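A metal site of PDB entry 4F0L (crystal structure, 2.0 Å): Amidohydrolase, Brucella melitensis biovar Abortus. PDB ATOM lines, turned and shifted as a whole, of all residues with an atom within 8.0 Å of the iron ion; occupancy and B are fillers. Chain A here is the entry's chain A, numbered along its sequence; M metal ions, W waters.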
ATOM      1  N   HIS A  65      -3.002 -10.620 -21.595  1.00  0.00           N
ATOM      2  CA  HIS A  65      -3.024 -10.087 -20.227  1.00  0.00           C
ATOM      3  C   HIS A  65      -1.835  -9.191 -20.015  1.00  0.00           C
ATOM      4  O   HIS A  65      -0.678  -9.642 -20.105  1.00  0.00           O
ATOM      5  CB  HIS A  65      -2.988 -11.233 -19.245  1.00  0.00           C
ATOM      6  CG  HIS A  65      -3.172 -10.818 -17.821  1.00  0.00           C
ATOM      7  ND1 HIS A  65      -4.378 -10.481 -17.291  1.00  0.00           N
ATOM      8  CD2 HIS A  65      -2.241 -10.697 -16.792  1.00  0.00           C
ATOM      9  CE1 HIS A  65      -4.228 -10.168 -15.994  1.00  0.00           C
ATOM     10  NE2 HIS A  65      -2.920 -10.323 -15.675  1.00  0.00           N
ATOM     11  N   SER A  66      -2.126  -7.902 -19.795  1.00  0.00           N
ATOM     12  CA  SER A  66      -1.144  -6.839 -19.677  1.00  0.00           C
ATOM     13  C   SER A  66      -1.595  -5.838 -18.621  1.00  0.00           C
ATOM     14  O   SER A  66      -2.785  -5.473 -18.562  1.00  0.00           O
ATOM     15  CB  SER A  66      -0.939  -6.113 -21.040  1.00  0.00           C
ATOM     16  OG  SER A  66      -0.306  -4.841 -20.863  1.00  0.00           O
ATOM     17  N   HIS A  67      -0.649  -5.398 -17.786  1.00  0.00           N
ATOM     18  CA  HIS A  67      -0.806  -4.177 -16.988  1.00  0.00           C
ATOM     19  C   HIS A  67       0.192  -3.165 -17.458  1.00  0.00           C
ATOM     20  O   HIS A  67       1.384  -3.205 -17.078  1.00  0.00           O
ATOM     21  CB  HIS A  67      -0.611  -4.429 -15.500  1.00  0.00           C
ATOM     22  CG  HIS A  67      -1.276  -5.654 -15.019  1.00  0.00           C
ATOM     23  ND1 HIS A  67      -2.613  -5.829 -15.079  1.00  0.00           N
ATOM     24  CD2 HIS A  67      -0.742  -6.809 -14.483  1.00  0.00           C
ATOM     25  CE1 HIS A  67      -2.904  -7.069 -14.571  1.00  0.00           C
ATOM     26  NE2 HIS A  67      -1.763  -7.641 -14.199  1.00  0.00           N
ATOM     27  N   GLN A  70       3.111  -1.268 -15.539  1.00  0.00           N
ATOM     28  CA  GLN A  70       4.216  -2.078 -14.971  1.00  0.00           C
ATOM     29  C   GLN A  70       5.402  -2.205 -15.889  1.00  0.00           C
ATOM     30  O   GLN A  70       6.528  -2.481 -15.430  1.00  0.00           O
ATOM     31  CB  GLN A  70       3.710  -3.467 -14.521  1.00  0.00           C
ATOM     32  CG  GLN A  70       2.710  -3.344 -13.358  1.00  0.00           C
ATOM     33  CD  GLN A  70       2.147  -4.661 -12.870  1.00  0.00           C
ATOM     34  OE1 GLN A  70       2.607  -5.740 -13.272  1.00  0.00           O
ATOM     35  NE2 GLN A  70       1.137  -4.609 -11.997  1.00  0.00           N
ATOM     36  N   TRP A  90       9.279  -5.954  -4.985  1.00  0.00           N
ATOM     37  CA  TRP A  90       8.369  -5.878  -6.142  1.00  0.00           C
ATOM     38  C   TRP A  90       7.142  -5.017  -5.842  1.00  0.00           C
ATOM     39  O   TRP A  90       6.803  -4.131  -6.601  1.00  0.00           O
ATOM     40  CB  TRP A  90       7.926  -7.272  -6.574  1.00  0.00           C
ATOM     41  CG  TRP A  90       7.240  -7.290  -7.908  1.00  0.00           C
ATOM     42  CD1 TRP A  90       7.814  -7.489  -9.165  1.00  0.00           C
ATOM     43  CD2 TRP A  90       5.802  -7.076  -8.163  1.00  0.00           C
ATOM     44  NE1 TRP A  90       6.852  -7.432 -10.156  1.00  0.00           N
ATOM     45  CE2 TRP A  90       5.621  -7.178  -9.624  1.00  0.00           C
ATOM     46  CE3 TRP A  90       4.701  -6.825  -7.352  1.00  0.00           C
ATOM     47  CZ2 TRP A  90       4.370  -7.032 -10.210  1.00  0.00           C
ATOM     48  CZ3 TRP A  90       3.449  -6.674  -7.962  1.00  0.00           C
ATOM     49  CH2 TRP A  90       3.290  -6.786  -9.368  1.00  0.00           C
ATOM     50  N   PHE A 128      -5.667  -5.453 -18.906  1.00  0.00           N
ATOM     51  CA  PHE A 128      -6.342  -5.792 -17.668  1.00  0.00           C
ATOM     52  C   PHE A 128      -6.074  -4.598 -16.807  1.00  0.00           C
ATOM     53  O   PHE A 128      -5.043  -4.494 -16.104  1.00  0.00           O
ATOM     54  CB  PHE A 128      -5.727  -7.080 -17.128  1.00  0.00           C
ATOM     55  CG  PHE A 128      -6.443  -7.726 -15.967  1.00  0.00           C
ATOM     56  CD1 PHE A 128      -6.272  -7.281 -14.689  1.00  0.00           C
ATOM     57  CD2 PHE A 128      -7.190  -8.876 -16.144  1.00  0.00           C
ATOM     58  CE1 PHE A 128      -6.886  -7.913 -13.598  1.00  0.00           C
ATOM     59  CE2 PHE A 128      -7.788  -9.519 -15.069  1.00  0.00           C
ATOM     60  CZ  PHE A 128      -7.639  -9.043 -13.788  1.00  0.00           C
ATOM     61  N   TYR A 130      -6.470  -1.660 -14.196  1.00  0.00           N
ATOM     62  CA  TYR A 130      -6.964  -1.285 -12.858  1.00  0.00           C
ATOM     63  C   TYR A 130      -6.485   0.051 -12.297  1.00  0.00           C
ATOM     64  O   TYR A 130      -6.853   0.404 -11.184  1.00  0.00           O
ATOM     65  CB  TYR A 130      -6.724  -2.381 -11.823  1.00  0.00           C
ATOM     66  CG  TYR A 130      -5.325  -2.852 -11.591  1.00  0.00           C
ATOM     67  CD1 TYR A 130      -4.460  -2.139 -10.780  1.00  0.00           C
ATOM     68  CD2 TYR A 130      -4.871  -4.040 -12.123  1.00  0.00           C
ATOM     69  CE1 TYR A 130      -3.175  -2.597 -10.501  1.00  0.00           C
ATOM     70  CE2 TYR A 130      -3.577  -4.484 -11.896  1.00  0.00           C
ATOM     71  CZ  TYR A 130      -2.744  -3.772 -11.059  1.00  0.00           C
ATOM     72  OH  TYR A 130      -1.490  -4.218 -10.809  1.00  0.00           O
ATOM     73  N   HIS A 216     -10.991  -8.432 -10.373  1.00  0.00           N
ATOM     74  CA  HIS A 216      -9.565  -8.565 -10.166  1.00  0.00           C
ATOM     75  C   HIS A 216      -9.148  -9.971  -9.758  1.00  0.00           C
ATOM     76  O   HIS A 216      -8.229 -10.577 -10.363  1.00  0.00           O
ATOM     77  CB  HIS A 216      -9.089  -7.574  -9.159  1.00  0.00           C
ATOM     78  CG  HIS A 216      -7.612  -7.638  -8.943  1.00  0.00           C
ATOM     79  ND1 HIS A 216      -7.058  -8.414  -7.983  1.00  0.00           N
ATOM     80  CD2 HIS A 216      -6.582  -7.045  -9.607  1.00  0.00           C
ATOM     81  CE1 HIS A 216      -5.731  -8.277  -8.012  1.00  0.00           C
ATOM     82  NE2 HIS A 216      -5.429  -7.433  -8.999  1.00  0.00           N
ATOM     83  N   ILE A 240     -10.195 -12.876 -14.930  1.00  0.00           N
ATOM     84  CA  ILE A 240     -10.012 -12.853 -13.479  1.00  0.00           C
ATOM     85  C   ILE A 240      -8.721 -13.555 -13.086  1.00  0.00           C
ATOM     86  O   ILE A 240      -8.414 -14.593 -13.649  1.00  0.00           O
ATOM     87  CB  ILE A 240     -11.197 -13.560 -12.780  1.00  0.00           C
ATOM     88  CG1 ILE A 240     -11.028 -13.532 -11.236  1.00  0.00           C
ATOM     89  CG2 ILE A 240     -11.435 -14.972 -13.362  1.00  0.00           C
ATOM     90  CD1 ILE A 240     -12.353 -13.733 -10.504  1.00  0.00           C
ATOM     91  N   HIS A 241      -7.933 -12.966 -12.164  1.00  0.00           N
ATOM     92  CA  HIS A 241      -6.738 -13.647 -11.657  1.00  0.00           C
ATOM     93  C   HIS A 241      -7.208 -14.740 -10.749  1.00  0.00           C
ATOM     94  O   HIS A 241      -7.980 -14.464  -9.843  1.00  0.00           O
ATOM     95  CB  HIS A 241      -5.846 -12.737 -10.796  1.00  0.00           C
ATOM     96  CG  HIS A 241      -5.101 -11.640 -11.525  1.00  0.00           C
ATOM     97  ND1 HIS A 241      -5.226 -10.326 -11.179  1.00  0.00           N
ATOM     98  CD2 HIS A 241      -4.109 -11.685 -12.521  1.00  0.00           C
ATOM     99  CE1 HIS A 241      -4.370  -9.569 -11.939  1.00  0.00           C
ATOM    100  NE2 HIS A 241      -3.726 -10.394 -12.789  1.00  0.00           N
ATOM    101  N   GLU A 244      -2.852 -17.836  -8.490  1.00  0.00           N
ATOM    102  CA  GLU A 244      -1.520 -17.517  -8.948  1.00  0.00           C
ATOM    103  C   GLU A 244      -0.447 -17.906  -7.928  1.00  0.00           C
ATOM    104  O   GLU A 244       0.596 -18.472  -8.317  1.00  0.00           O
ATOM    105  CB  GLU A 244      -1.377 -16.021  -9.305  1.00  0.00           C
ATOM    106  CG  GLU A 244       0.026 -15.693  -9.837  1.00  0.00           C
ATOM    107  CD  GLU A 244       0.271 -14.196 -10.125  1.00  0.00           C
ATOM    108  OE1 GLU A 244       1.393 -13.831 -10.561  1.00  0.00           O
ATOM    109  OE2 GLU A 244      -0.660 -13.397  -9.934  1.00  0.00           O
ATOM    110  N   ILE A 277      -6.732 -16.161 -15.397  1.00  0.00           N
ATOM    111  CA  ILE A 277      -5.333 -15.773 -15.490  1.00  0.00           C
ATOM    112  C   ILE A 277      -4.479 -16.562 -14.477  1.00  0.00           C
ATOM    113  O   ILE A 277      -4.819 -16.630 -13.291  1.00  0.00           O
ATOM    114  CB  ILE A 277      -5.163 -14.253 -15.292  1.00  0.00           C
ATOM    115  CG1 ILE A 277      -6.140 -13.475 -16.174  1.00  0.00           C
ATOM    116  CG2 ILE A 277      -3.720 -13.835 -15.639  1.00  0.00           C
ATOM    117  CD1 ILE A 277      -5.969 -13.705 -17.668  1.00  0.00           C
ATOM    118  N   HIS A 278      -3.372 -17.101 -14.953  1.00  0.00           N
ATOM    119  CA  HIS A 278      -2.453 -17.962 -14.203  1.00  0.00           C
ATOM    120  C   HIS A 278      -2.989 -19.361 -13.961  1.00  0.00           C
ATOM    121  O   HIS A 278      -2.532 -20.323 -14.632  1.00  0.00           O
ATOM    122  CB  HIS A 278      -1.987 -17.284 -12.903  1.00  0.00           C
ATOM    123  CG  HIS A 278      -1.454 -15.924 -13.110  1.00  0.00           C
ATOM    124  ND1 HIS A 278      -0.399 -15.664 -13.914  1.00  0.00           N
ATOM    125  CD2 HIS A 278      -1.869 -14.669 -12.589  1.00  0.00           C
ATOM    126  CE1 HIS A 278      -0.129 -14.346 -13.908  1.00  0.00           C
ATOM    127  NE2 HIS A 278      -1.042 -13.732 -13.119  1.00  0.00           N
ATOM    128  N   GLY A 298      -5.174 -18.137 -19.089  1.00  0.00           N
ATOM    129  CA  GLY A 298      -4.408 -16.953 -19.443  1.00  0.00           C
ATOM    130  C   GLY A 298      -3.046 -17.116 -18.813  1.00  0.00           C
ATOM    131  O   GLY A 298      -2.821 -16.693 -17.680  1.00  0.00           O
ATOM    132  N   CYS A 300       0.922 -16.684 -18.146  1.00  0.00           N
ATOM    133  CA  CYS A 300       1.894 -15.595 -18.173  1.00  0.00           C
ATOM    134  C   CYS A 300       3.256 -16.138 -17.731  1.00  0.00           C
ATOM    135  O   CYS A 300       3.729 -15.836 -16.640  1.00  0.00           O
ATOM    136  CB  CYS A 300       1.429 -14.476 -17.270  1.00  0.00           C
ATOM    137  SG  CYS A 300      -0.227 -13.864 -17.663  1.00  0.00           S
ATOM    138  N   THR A 303       6.304 -13.792 -16.447  1.00  0.00           N
ATOM    139  CA  THR A 303       5.974 -13.112 -15.215  1.00  0.00           C
ATOM    140  C   THR A 303       5.869 -14.115 -14.079  1.00  0.00           C
ATOM    141  O   THR A 303       6.334 -13.853 -12.969  1.00  0.00           O
ATOM    142  CB  THR A 303       4.690 -12.278 -15.336  1.00  0.00           C
ATOM    143  OG1 THR A 303       4.915 -11.226 -16.306  1.00  0.00           O
ATOM    144  CG2 THR A 303       4.346 -11.680 -13.960  1.00  0.00           C
ATOM    145  N   LEU A 307       8.112 -13.901 -10.762  1.00  0.00           N
ATOM    146  CA  LEU A 307       7.483 -13.792  -9.451  1.00  0.00           C
ATOM    147  C   LEU A 307       7.590 -15.078  -8.582  1.00  0.00           C
ATOM    148  O   LEU A 307       7.180 -15.088  -7.431  1.00  0.00           O
ATOM    149  CB  LEU A 307       6.005 -13.386  -9.619  1.00  0.00           C
ATOM    150  CG  LEU A 307       5.757 -12.022 -10.277  1.00  0.00           C
ATOM    151  CD1 LEU A 307       4.260 -11.749 -10.372  1.00  0.00           C
ATOM    152  CD2 LEU A 307       6.516 -10.929  -9.508  1.00  0.00           C
ATOM    153  N   GLY A 327       0.178 -13.986 -21.996  1.00  0.00           N
ATOM    154  CA  GLY A 327       0.247 -12.570 -21.706  1.00  0.00           C
ATOM    155  C   GLY A 327       1.526 -12.142 -21.019  1.00  0.00           C
ATOM    156  O   GLY A 327       2.056 -12.837 -20.164  1.00  0.00           O
ATOM    157  N   SER A 328       2.023 -10.958 -21.397  1.00  0.00           N
ATOM    158  CA  SER A 328       3.250 -10.412 -20.822  1.00  0.00           C
ATOM    159  C   SER A 328       3.075  -9.922 -19.360  1.00  0.00           C
ATOM    160  O   SER A 328       4.059  -9.814 -18.645  1.00  0.00           O
ATOM    161  CB  SER A 328       3.751  -9.260 -21.696  1.00  0.00           C
ATOM    162  OG  SER A 328       4.120  -9.754 -22.964  1.00  0.00           O
ATOM    163  N   ASP A 329       1.829  -9.586 -18.982  1.00  0.00           N
ATOM    164  CA  ASP A 329       1.407  -9.431 -17.593  1.00  0.00           C
ATOM    165  C   ASP A 329       2.125  -8.274 -16.909  1.00  0.00           C
ATOM    166  O   ASP A 329       1.713  -7.133 -17.086  1.00  0.00           O
ATOM    167  CB  ASP A 329       1.535 -10.767 -16.839  1.00  0.00           C
ATOM    168  CG  ASP A 329       0.967 -10.704 -15.406  1.00  0.00           C
ATOM    169  OD1 ASP A 329       0.393  -9.647 -15.014  1.00  0.00           O
ATOM    170  OD2 ASP A 329       1.120 -11.695 -14.671  1.00  0.00           O
ATOM    171  N   SER A 330       3.249  -8.564 -16.220  1.00  0.00           N
ATOM    172  CA  SER A 330       4.061  -7.520 -15.592  1.00  0.00           C
ATOM    173  C   SER A 330       4.831  -6.703 -16.606  1.00  0.00           C
ATOM    174  O   SER A 330       5.366  -5.629 -16.291  1.00  0.00           O
ATOM    175  CB  SER A 330       5.057  -8.108 -14.548  1.00  0.00           C
ATOM    176  OG  SER A 330       6.113  -8.834 -15.183  1.00  0.00           O
HETATM  177 FE    FE M   1      -1.727  -9.824 -13.873  1.00  0.00          FE
HETATM  178  O   HOH W   1      -0.551  -9.028 -11.808  1.00  0.00           O
HETATM  179  O   HOH W   2      -1.035 -11.407 -13.070  1.00  0.00           O
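ND1 of His 67 lies within hydrogen-bond range of O of Phe 128 (3.0 Å). The backbone NH (N) of Ser 328 is in hydrogen-bond range of the backbone carbonyl oxygen (O) of His 65, 3.3 Å away. The backbone carbonyl oxygen (O) of His 216 sits at hydrogen-bond distance from the backbone NH (N) of His 241 (3.0 Å). A ring nitrogen (NE2) of His 278 lies close to the side-chain carboxylate (OD2) of Asp 329.
The iron ion is bound by water W2. The iron ion is bound by a ring nitrogen (NE2) of His 67, at 2.2 Å. NE2 of His 65 is bound to the iron ion, at 2.2 Å. A ring nitrogen (NE2) of His 241 is bound to the iron ion. The iron ion is bound by OD1 of Asp 329, 2.4 Å away. The iron ion is bound by water W1. The iron ion has six donor atoms within binding distance.
Of the 21 residues printed, 4 come within 4 Å of the iron ion.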
